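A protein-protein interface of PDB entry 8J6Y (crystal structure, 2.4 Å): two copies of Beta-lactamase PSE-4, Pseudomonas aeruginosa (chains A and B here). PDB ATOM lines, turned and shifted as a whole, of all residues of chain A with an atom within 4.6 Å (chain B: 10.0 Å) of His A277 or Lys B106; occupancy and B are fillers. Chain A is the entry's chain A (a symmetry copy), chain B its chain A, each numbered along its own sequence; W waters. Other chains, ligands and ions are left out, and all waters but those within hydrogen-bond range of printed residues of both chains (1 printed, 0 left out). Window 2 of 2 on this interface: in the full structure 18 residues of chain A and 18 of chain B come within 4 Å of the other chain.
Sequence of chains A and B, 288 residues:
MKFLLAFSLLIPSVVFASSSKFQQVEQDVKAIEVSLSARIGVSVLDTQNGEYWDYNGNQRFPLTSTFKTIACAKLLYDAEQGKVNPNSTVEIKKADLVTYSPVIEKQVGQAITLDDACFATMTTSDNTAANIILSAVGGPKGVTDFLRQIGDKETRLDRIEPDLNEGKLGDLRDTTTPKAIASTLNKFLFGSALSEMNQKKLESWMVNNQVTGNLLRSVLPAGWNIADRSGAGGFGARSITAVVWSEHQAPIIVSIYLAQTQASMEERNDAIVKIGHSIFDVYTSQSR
ND1 of His A277 lies within hydrogen-bond range of OE1 of Glu B105 (3.1 Å). The side-chain amino group (NZ) of Lys B106 lies within hydrogen-bond range of the backbone carbonyl oxygen (O) of Val A219 (2.8 Å).
A ring nitrogen (NE2) of His A277 sits at hydrogen-bond distance from the side-chain carboxylate (OD1) of Asp A281 (3.5 Å).
O of Pro B102 touches CG1 of Val A219, at 3.6 Å. Tyr B100 touches Val A273. OE2 of Glu B105 touches CG2 of Val A273 (3.9 Å). Lys A274 touches Glu B105. Lys B106 touches His A277.
His A277 touches just these residues of chain B: Glu B105 and Lys B106. Lys B106 touches two residues of chain A. Val A219 touches just these residues of chain B: Pro B102 (3.6 Å) and Lys B106 (2.8 Å). No residue of chain B comes within 4 Å of Gly A276. No residue of chain B comes within 4 Å of Ser A278. Of the printed residues of chain A, Tyr B100 touches Val A273 (3.98 Å). Printed residues of chain B within 4 Å of Val A273: Tyr B100 and Glu B105. The nearest residue of chain B that does not touch His A277 is Gln B107 (6.0 Å).
Of the 11 printed residues of chain A, 4 touch a printed residue of chain B. Hydrophobic or aromatic side chains of chain A that line the printed part of chain B: Val A219, Val A273 and His A277. Hydrophobic or aromatic side chains of chain B that line the printed part of chain A: Tyr B100 and Pro B102. Along chain B the printed residues that touch a printed residue of chain A span positions 100 to 106. Among the printed residues, 7 pairs touch across the chains. Among the printed residues, no Asp or Glu carboxylate lies within 4 Å of a Lys or Arg side-chain nitrogen of the other chain.
No position is printed for both chains. Of the 7 pairs that touch across the chains among the printed residues, none has its exchanged pair printed and touching as well.
Water W1 bridges the side-chain carboxylate of Asp A281 (2.9 Å) and the side-chain amino group of Lys B106 (3.2 Å).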
ATOM      1  N   VAL A 219       2.187   3.459   9.854  1.00  0.00           N
ATOM      2  CA  VAL A 219       0.798   3.842  10.092  1.00  0.00           C
ATOM      3  C   VAL A 219       0.416   5.028   9.199  1.00  0.00           C
ATOM      4  O   VAL A 219      -0.584   5.683   9.435  1.00  0.00           O
ATOM      5  CB  VAL A 219       0.542   4.169  11.579  1.00  0.00           C
ATOM      6  CG1 VAL A 219       0.510   2.931  12.443  1.00  0.00           C
ATOM      7  CG2 VAL A 219       1.544   5.169  12.142  1.00  0.00           C
ATOM      8  N   PRO A 221      -1.380   7.135   6.424  1.00  0.00           N
ATOM      9  CA  PRO A 221      -2.592   6.970   5.618  1.00  0.00           C
ATOM     10  C   PRO A 221      -2.240   6.692   4.155  1.00  0.00           C
ATOM     11  O   PRO A 221      -1.177   7.114   3.684  1.00  0.00           O
ATOM     12  CB  PRO A 221      -3.344   8.306   5.750  1.00  0.00           C
ATOM     13  CG  PRO A 221      -2.818   8.906   7.041  1.00  0.00           C
ATOM     14  CD  PRO A 221      -1.376   8.444   7.107  1.00  0.00           C
ATOM     15  N   VAL A 273       4.181   4.531  17.152  1.00  0.00           N
ATOM     16  CA  VAL A 273       3.232   4.316  16.063  1.00  0.00           C
ATOM     17  C   VAL A 273       1.798   4.537  16.547  1.00  0.00           C
ATOM     18  O   VAL A 273       0.904   4.821  15.749  1.00  0.00           O
ATOM     19  CB  VAL A 273       3.380   2.935  15.403  1.00  0.00           C
ATOM     20  CG1 VAL A 273       4.816   2.652  15.008  1.00  0.00           C
ATOM     21  CG2 VAL A 273       2.857   1.836  16.283  1.00  0.00           C
ATOM     22  N   LYS A 274       1.564   4.339  17.845  1.00  0.00           N
ATOM     23  CA  LYS A 274       0.289   4.679  18.465  1.00  0.00           C
ATOM     24  C   LYS A 274       0.046   6.194  18.444  1.00  0.00           C
ATOM     25  O   LYS A 274      -1.007   6.652  18.002  1.00  0.00           O
ATOM     26  CB  LYS A 274       0.273   4.176  19.905  1.00  0.00           C
ATOM     27  CG  LYS A 274      -0.097   2.719  20.055  1.00  0.00           C
ATOM     28  CD  LYS A 274       0.031   2.200  21.470  1.00  0.00           C
ATOM     29  CE  LYS A 274      -0.778   0.939  21.665  1.00  0.00           C
ATOM     30  NZ  LYS A 274       0.033  -0.091  22.349  1.00  0.00           N
ATOM     31  N   ILE A 275       1.043   6.955  18.915  1.00  0.00           N
ATOM     32  CA  ILE A 275       0.991   8.404  18.922  1.00  0.00           C
ATOM     33  C   ILE A 275       0.867   8.932  17.493  1.00  0.00           C
ATOM     34  O   ILE A 275       0.108   9.843  17.247  1.00  0.00           O
ATOM     35  CB  ILE A 275       2.198   8.980  19.676  1.00  0.00           C
ATOM     36  CG1 ILE A 275       2.130   8.596  21.154  1.00  0.00           C
ATOM     37  CG2 ILE A 275       2.259  10.483  19.534  1.00  0.00           C
ATOM     38  CD1 ILE A 275       3.323   9.054  21.962  1.00  0.00           C
ATOM     39  N   GLY A 276       1.586   8.346  16.542  1.00  0.00           N
ATOM     40  CA  GLY A 276       1.503   8.779  15.157  1.00  0.00           C
ATOM     41  C   GLY A 276       0.101   8.585  14.569  1.00  0.00           C
ATOM     42  O   GLY A 276      -0.403   9.424  13.846  1.00  0.00           O
ATOM     43  N   HIS A 277      -0.511   7.462  14.912  1.00  0.00           N
ATOM     44  CA  HIS A 277      -1.798   7.088  14.380  1.00  0.00           C
ATOM     45  C   HIS A 277      -2.887   8.027  14.926  1.00  0.00           C
ATOM     46  O   HIS A 277      -3.765   8.452  14.180  1.00  0.00           O
ATOM     47  CB  HIS A 277      -1.992   5.610  14.708  1.00  0.00           C
ATOM     48  CG  HIS A 277      -3.383   5.155  14.556  1.00  0.00           C
ATOM     49  ND1 HIS A 277      -3.981   4.318  15.480  1.00  0.00           N
ATOM     50  CD2 HIS A 277      -4.276   5.400  13.579  1.00  0.00           C
ATOM     51  CE1 HIS A 277      -5.220   4.082  15.081  1.00  0.00           C
ATOM     52  NE2 HIS A 277      -5.419   4.738  13.928  1.00  0.00           N
ATOM     53  N   SER A 278      -2.845   8.318  16.235  1.00  0.00           N
ATOM     54  CA  SER A 278      -3.702   9.347  16.811  1.00  0.00           C
ATOM     55  C   SER A 278      -3.494  10.676  16.090  1.00  0.00           C
ATOM     56  O   SER A 278      -4.469  11.351  15.782  1.00  0.00           O
ATOM     57  CB  SER A 278      -3.432   9.557  18.249  1.00  0.00           C
ATOM     58  OG  SER A 278      -3.899   8.464  18.984  1.00  0.00           O
ATOM     59  N   ILE A 279      -2.226  11.058  15.868  1.00  0.00           N
ATOM     60  CA  ILE A 279      -1.973  12.339  15.254  1.00  0.00           C
ATOM     61  C   ILE A 279      -2.563  12.306  13.855  1.00  0.00           C
ATOM     62  O   ILE A 279      -3.258  13.233  13.477  1.00  0.00           O
ATOM     63  CB  ILE A 279      -0.485  12.721  15.286  1.00  0.00           C
ATOM     64  CG1 ILE A 279      -0.013  12.928  16.733  1.00  0.00           C
ATOM     65  CG2 ILE A 279      -0.219  13.947  14.424  1.00  0.00           C
ATOM     66  CD1 ILE A 279       1.476  12.873  16.899  1.00  0.00           C
ATOM     67  N   PHE A 280      -2.347  11.208  13.132  1.00  0.00           N
ATOM     68  CA  PHE A 280      -2.787  11.150  11.761  1.00  0.00           C
ATOM     69  C   PHE A 280      -4.310  11.210  11.705  1.00  0.00           C
ATOM     70  O   PHE A 280      -4.824  11.824  10.776  1.00  0.00           O
ATOM     71  CB  PHE A 280      -2.246   9.899  11.089  1.00  0.00           C
ATOM     72  CG  PHE A 280      -0.781   9.955  10.763  1.00  0.00           C
ATOM     73  CD1 PHE A 280      -0.114  11.172  10.662  1.00  0.00           C
ATOM     74  CD2 PHE A 280      -0.056   8.781  10.613  1.00  0.00           C
ATOM     75  CE1 PHE A 280       1.249  11.213  10.420  1.00  0.00           C
ATOM     76  CE2 PHE A 280       1.298   8.819  10.342  1.00  0.00           C
ATOM     77  CZ  PHE A 280       1.947  10.034  10.238  1.00  0.00           C
ATOM     78  N   ASP A 281      -4.975  10.557  12.677  1.00  0.00           N
ATOM     79  CA  ASP A 281      -6.429  10.457  12.788  1.00  0.00           C
ATOM     80  C   ASP A 281      -7.108  11.812  12.890  1.00  0.00           C
ATOM     81  O   ASP A 281      -8.245  11.995  12.451  1.00  0.00           O
ATOM     82  CB  ASP A 281      -6.877   9.807  14.092  1.00  0.00           C
ATOM     83  CG  ASP A 281      -7.051   8.311  13.993  1.00  0.00           C
ATOM     84  OD1 ASP A 281      -6.751   7.767  12.931  1.00  0.00           O
ATOM     85  OD2 ASP A 281      -7.502   7.711  14.982  1.00  0.00           O
ATOM     86  N   ILE B  92     -11.245  -7.908  13.813  1.00  0.00           N
ATOM     87  CA  ILE B  92     -10.304  -7.465  14.823  1.00  0.00           C
ATOM     88  C   ILE B  92     -11.081  -6.872  15.988  1.00  0.00           C
ATOM     89  O   ILE B  92     -11.803  -5.895  15.817  1.00  0.00           O
ATOM     90  CB  ILE B  92      -9.313  -6.438  14.233  1.00  0.00           C
ATOM     91  CG1 ILE B  92      -8.694  -6.911  12.907  1.00  0.00           C
ATOM     92  CG2 ILE B  92      -8.252  -6.088  15.270  1.00  0.00           C
ATOM     93  CD1 ILE B  92      -8.295  -5.792  11.966  1.00  0.00           C
ATOM     94  N   LYS B  93     -10.893  -7.441  17.178  1.00  0.00           N
ATOM     95  CA  LYS B  93     -11.425  -6.841  18.391  1.00  0.00           C
ATOM     96  C   LYS B  93     -10.293  -6.136  19.139  1.00  0.00           C
ATOM     97  O   LYS B  93      -9.155  -6.608  19.159  1.00  0.00           O
ATOM     98  CB  LYS B  93     -12.091  -7.901  19.276  1.00  0.00           C
ATOM     99  CG  LYS B  93     -13.287  -8.601  18.643  1.00  0.00           C
ATOM    100  CD  LYS B  93     -13.642  -9.904  19.319  1.00  0.00           C
ATOM    101  CE  LYS B  93     -15.063 -10.352  19.052  1.00  0.00           C
ATOM    102  NZ  LYS B  93     -15.526 -11.313  20.082  1.00  0.00           N
ATOM    103  N   LYS B  94     -10.641  -5.015  19.781  1.00  0.00           N
ATOM    104  CA  LYS B  94      -9.718  -4.248  20.599  1.00  0.00           C
ATOM    105  C   LYS B  94      -8.907  -5.176  21.518  1.00  0.00           C
ATOM    106  O   LYS B  94      -7.691  -5.021  21.619  1.00  0.00           O
ATOM    107  CB  LYS B  94     -10.468  -3.163  21.388  1.00  0.00           C
ATOM    108  CG  LYS B  94      -9.762  -1.810  21.429  1.00  0.00           C
ATOM    109  CD  LYS B  94     -10.192  -0.869  22.545  1.00  0.00           C
ATOM    110  CE  LYS B  94      -9.569   0.509  22.421  1.00  0.00           C
ATOM    111  NZ  LYS B  94      -9.823   1.350  23.614  1.00  0.00           N
ATOM    112  N   LEU B  97      -5.494  -7.095  20.581  1.00  0.00           N
ATOM    113  CA  LEU B  97      -4.283  -6.346  20.274  1.00  0.00           C
ATOM    114  C   LEU B  97      -3.165  -6.644  21.280  1.00  0.00           C
ATOM    115  O   LEU B  97      -3.393  -6.746  22.488  1.00  0.00           O
ATOM    116  CB  LEU B  97      -4.599  -4.844  20.189  1.00  0.00           C
ATOM    117  CG  LEU B  97      -5.408  -4.401  18.961  1.00  0.00           C
ATOM    118  CD1 LEU B  97      -5.734  -2.915  19.013  1.00  0.00           C
ATOM    119  CD2 LEU B  97      -4.677  -4.696  17.663  1.00  0.00           C
ATOM    120  N   VAL B  98      -1.954  -6.825  20.716  1.00  0.00           N
ATOM    121  CA  VAL B  98      -0.718  -6.994  21.459  1.00  0.00           C
ATOM    122  C   VAL B  98       0.228  -5.878  21.024  1.00  0.00           C
ATOM    123  O   VAL B  98       0.042  -5.253  19.981  1.00  0.00           O
ATOM    124  CB  VAL B  98      -0.095  -8.390  21.218  1.00  0.00           C
ATOM    125  CG1 VAL B  98      -1.020  -9.511  21.679  1.00  0.00           C
ATOM    126  CG2 VAL B  98       0.306  -8.620  19.761  1.00  0.00           C
ATOM    127  N   TYR B 100       2.968  -3.638  19.474  1.00  0.00           N
ATOM    128  CA  TYR B 100       3.464  -3.413  18.123  1.00  0.00           C
ATOM    129  C   TYR B 100       2.647  -4.166  17.072  1.00  0.00           C
ATOM    130  O   TYR B 100       3.035  -5.234  16.591  1.00  0.00           O
ATOM    131  CB  TYR B 100       4.947  -3.721  17.950  1.00  0.00           C
ATOM    132  CG  TYR B 100       5.486  -3.060  16.704  1.00  0.00           C
ATOM    133  CD1 TYR B 100       5.750  -1.697  16.657  1.00  0.00           C
ATOM    134  CD2 TYR B 100       5.587  -3.772  15.528  1.00  0.00           C
ATOM    135  CE1 TYR B 100       6.132  -1.073  15.478  1.00  0.00           C
ATOM    136  CE2 TYR B 100       6.011  -3.171  14.358  1.00  0.00           C
ATOM    137  CZ  TYR B 100       6.265  -1.822  14.323  1.00  0.00           C
ATOM    138  OH  TYR B 100       6.706  -1.329  13.125  1.00  0.00           O
ATOM    139  N   SER B 101       1.538  -3.520  16.701  1.00  0.00           N
ATOM    140  CA  SER B 101       0.631  -3.919  15.640  1.00  0.00           C
ATOM    141  C   SER B 101       0.243  -2.672  14.854  1.00  0.00           C
ATOM    142  O   SER B 101      -0.858  -2.174  14.994  1.00  0.00           O
ATOM    143  CB  SER B 101      -0.610  -4.575  16.179  1.00  0.00           C
ATOM    144  OG  SER B 101      -0.293  -5.670  16.996  1.00  0.00           O
ATOM    145  N   PRO B 102       1.142  -2.084  14.054  1.00  0.00           N
ATOM    146  CA  PRO B 102       0.799  -0.870  13.307  1.00  0.00           C
ATOM    147  C   PRO B 102      -0.408  -1.009  12.369  1.00  0.00           C
ATOM    148  O   PRO B 102      -1.280  -0.143  12.335  1.00  0.00           O
ATOM    149  CB  PRO B 102       2.072  -0.553  12.503  1.00  0.00           C
ATOM    150  CG  PRO B 102       2.958  -1.803  12.608  1.00  0.00           C
ATOM    151  CD  PRO B 102       2.529  -2.537  13.858  1.00  0.00           C
ATOM    152  N   VAL B 103      -0.440  -2.092  11.591  1.00  0.00           N
ATOM    153  CA  VAL B 103      -1.474  -2.283  10.581  1.00  0.00           C
ATOM    154  C   VAL B 103      -2.811  -2.577  11.257  1.00  0.00           C
ATOM    155  O   VAL B 103      -3.858  -2.022  10.920  1.00  0.00           O
ATOM    156  CB  VAL B 103      -1.081  -3.429   9.639  1.00  0.00           C
ATOM    157  CG1 VAL B 103      -2.211  -3.838   8.704  1.00  0.00           C
ATOM    158  CG2 VAL B 103       0.153  -3.046   8.858  1.00  0.00           C
ATOM    159  N   ILE B 104      -2.768  -3.464  12.234  1.00  0.00           N
ATOM    160  CA  ILE B 104      -4.000  -4.009  12.744  1.00  0.00           C
ATOM    161  C   ILE B 104      -4.644  -3.009  13.699  1.00  0.00           C
ATOM    162  O   ILE B 104      -5.860  -3.002  13.840  1.00  0.00           O
ATOM    163  CB  ILE B 104      -3.737  -5.370  13.401  1.00  0.00           C
ATOM    164  CG1 ILE B 104      -3.097  -6.367  12.428  1.00  0.00           C
ATOM    165  CG2 ILE B 104      -5.009  -5.914  13.997  1.00  0.00           C
ATOM    166  CD1 ILE B 104      -3.981  -6.769  11.260  1.00  0.00           C
ATOM    167  N   GLU B 105      -3.856  -2.165  14.367  1.00  0.00           N
ATOM    168  CA  GLU B 105      -4.445  -1.198  15.288  1.00  0.00           C
ATOM    169  C   GLU B 105      -5.200  -0.115  14.518  1.00  0.00           C
ATOM    170  O   GLU B 105      -6.022   0.566  15.119  1.00  0.00           O
ATOM    171  CB  GLU B 105      -3.412  -0.572  16.232  1.00  0.00           C
ATOM    172  CG  GLU B 105      -2.508   0.452  15.587  1.00  0.00           C
ATOM    173  CD  GLU B 105      -1.668   1.189  16.612  1.00  0.00           C
ATOM    174  OE1 GLU B 105      -1.971   2.374  16.853  1.00  0.00           O
ATOM    175  OE2 GLU B 105      -0.725   0.574  17.172  1.00  0.00           O
ATOM    176  N   LYS B 106      -4.903   0.049  13.216  1.00  0.00           N
ATOM    177  CA  LYS B 106      -5.651   0.947  12.352  1.00  0.00           C
ATOM    178  C   LYS B 106      -7.011   0.364  11.962  1.00  0.00           C
ATOM    179  O   LYS B 106      -7.726   1.004  11.209  1.00  0.00           O
ATOM    180  CB  LYS B 106      -4.921   1.239  11.034  1.00  0.00           C
ATOM    181  CG  LYS B 106      -3.515   1.829  11.128  1.00  0.00           C
ATOM    182  CD  LYS B 106      -3.196   2.882  10.062  1.00  0.00           C
ATOM    183  CE  LYS B 106      -4.047   4.129  10.219  1.00  0.00           C
ATOM    184  NZ  LYS B 106      -3.290   5.395  10.033  1.00  0.00           N
ATOM    185  N   GLN B 107      -7.389  -0.836  12.431  1.00  0.00           N
ATOM    186  CA  GLN B 107      -8.501  -1.554  11.807  1.00  0.00           C
ATOM    187  C   GLN B 107      -9.413  -2.251  12.817  1.00  0.00           C
ATOM    188  O   GLN B 107     -10.188  -3.123  12.426  1.00  0.00           O
ATOM    189  CB  GLN B 107      -7.992  -2.586  10.792  1.00  0.00           C
ATOM    190  CG  GLN B 107      -7.527  -1.955   9.485  1.00  0.00           C
ATOM    191  CD  GLN B 107      -7.184  -3.023   8.480  1.00  0.00           C
ATOM    192  OE1 GLN B 107      -8.043  -3.808   8.086  1.00  0.00           O
ATOM    193  NE2 GLN B 107      -5.922  -3.090   8.082  1.00  0.00           N
ATOM    194  N   VAL B 108      -9.367  -1.844  14.091  1.00  0.00           N
ATOM    195  CA  VAL B 108     -10.299  -2.363  15.082  1.00  0.00           C
ATOM    196  C   VAL B 108     -11.731  -2.168  14.567  1.00  0.00           C
ATOM    197  O   VAL B 108     -12.080  -1.093  14.069  1.00  0.00           O
ATOM    198  CB  VAL B 108     -10.076  -1.685  16.445  1.00  0.00           C
ATOM    199  CG1 VAL B 108     -11.170  -2.033  17.444  1.00  0.00           C
ATOM    200  CG2 VAL B 108      -8.707  -2.031  16.997  1.00  0.00           C
ATOM    201  N   GLY B 109     -12.548  -3.231  14.663  1.00  0.00           N
ATOM    202  CA  GLY B 109     -13.880  -3.253  14.069  1.00  0.00           C
ATOM    203  C   GLY B 109     -13.881  -3.215  12.537  1.00  0.00           C
ATOM    204  O   GLY B 109     -14.839  -2.739  11.936  1.00  0.00           O
ATOM    205  N   GLN B 110     -12.812  -3.721  11.910  1.00  0.00           N
ATOM    206  CA  GLN B 110     -12.836  -4.117  10.508  1.00  0.00           C
ATOM    207  C   GLN B 110     -12.295  -5.544  10.369  1.00  0.00           C
ATOM    208  O   GLN B 110     -11.634  -6.061  11.286  1.00  0.00           O
ATOM    209  CB  GLN B 110     -11.981  -3.191   9.637  1.00  0.00           C
ATOM    210  CG  GLN B 110     -12.454  -1.753   9.574  1.00  0.00           C
ATOM    211  CD  GLN B 110     -11.462  -0.933   8.787  1.00  0.00           C
ATOM    212  OE1 GLN B 110     -11.187  -1.203   7.619  1.00  0.00           O
ATOM    213  NE2 GLN B 110     -10.882   0.062   9.439  1.00  0.00           N
ATOM    214  N   ALA B 111     -12.556  -6.138   9.190  1.00  0.00           N
ATOM    215  CA  ALA B 111     -12.126  -7.494   8.865  1.00  0.00           C
ATOM    216  C   ALA B 111     -10.891  -7.469   7.955  1.00  0.00           C
ATOM    217  O   ALA B 111     -10.684  -6.555   7.156  1.00  0.00           O
ATOM    218  CB  ALA B 111     -13.266  -8.256   8.230  1.00  0.00           C
ATOM    219  N   ILE B 112     -10.045  -8.488   8.079  1.00  0.00           N
ATOM    220  CA  ILE B 112      -8.874  -8.551   7.225  1.00  0.00           C
ATOM    221  C   ILE B 112      -8.775  -9.948   6.615  1.00  0.00           C
ATOM    222  O   ILE B 112      -9.029 -10.938   7.301  1.00  0.00           O
ATOM    223  CB  ILE B 112      -7.622  -8.139   8.023  1.00  0.00           C
ATOM    224  CG1 ILE B 112      -6.397  -7.995   7.115  1.00  0.00           C
ATOM    225  CG2 ILE B 112      -7.370  -9.083   9.193  1.00  0.00           C
ATOM    226  CD1 ILE B 112      -5.264  -7.181   7.729  1.00  0.00           C
ATOM    227  N   ALA B 120       0.929  -7.923   6.083  1.00  0.00           N
ATOM    228  CA  ALA B 120       1.201  -7.057   7.216  1.00  0.00           C
ATOM    229  C   ALA B 120       2.340  -7.622   8.058  1.00  0.00           C
ATOM    230  O   ALA B 120       3.313  -6.943   8.280  1.00  0.00           O
ATOM    231  CB  ALA B 120      -0.046  -6.898   8.057  1.00  0.00           C
ATOM    232  N   THR B 124       5.773  -5.581   7.993  1.00  0.00           N
ATOM    233  CA  THR B 124       5.956  -4.641   9.101  1.00  0.00           C
ATOM    234  C   THR B 124       6.253  -5.349  10.417  1.00  0.00           C
ATOM    235  O   THR B 124       6.639  -4.709  11.398  1.00  0.00           O
ATOM    236  CB  THR B 124       4.735  -3.759   9.355  1.00  0.00           C
ATOM    237  OG1 THR B 124       3.726  -4.601   9.923  1.00  0.00           O
ATOM    238  CG2 THR B 124       4.253  -3.030   8.115  1.00  0.00           C
ATOM    239  N   ASP B 126       3.891  -6.797  12.180  1.00  0.00           N
ATOM    240  CA  ASP B 126       2.734  -6.570  13.029  1.00  0.00           C
ATOM    241  C   ASP B 126       2.467  -7.830  13.833  1.00  0.00           C
ATOM    242  O   ASP B 126       2.347  -8.917  13.262  1.00  0.00           O
ATOM    243  CB  ASP B 126       1.533  -6.204  12.167  1.00  0.00           C
ATOM    244  CG  ASP B 126       0.310  -5.861  12.988  1.00  0.00           C
ATOM    245  OD1 ASP B 126      -0.030  -6.646  13.914  1.00  0.00           O
ATOM    246  OD2 ASP B 126      -0.261  -4.787  12.730  1.00  0.00           O
ATOM    247  N   THR B 128      -0.098  -8.574  16.030  1.00  0.00           N
ATOM    248  CA  THR B 128      -1.461  -9.055  16.099  1.00  0.00           C
ATOM    249  C   THR B 128      -1.754  -9.869  14.840  1.00  0.00           C
ATOM    250  O   THR B 128      -2.409 -10.896  14.909  1.00  0.00           O
ATOM    251  CB  THR B 128      -2.451  -7.910  16.310  1.00  0.00           C
ATOM    252  OG1 THR B 128      -2.113  -7.273  17.553  1.00  0.00           O
ATOM    253  CG2 THR B 128      -3.874  -8.432  16.306  1.00  0.00           C
HETATM  254  O   HOH W   1      -5.284   7.895  10.459  1.00  0.00           O
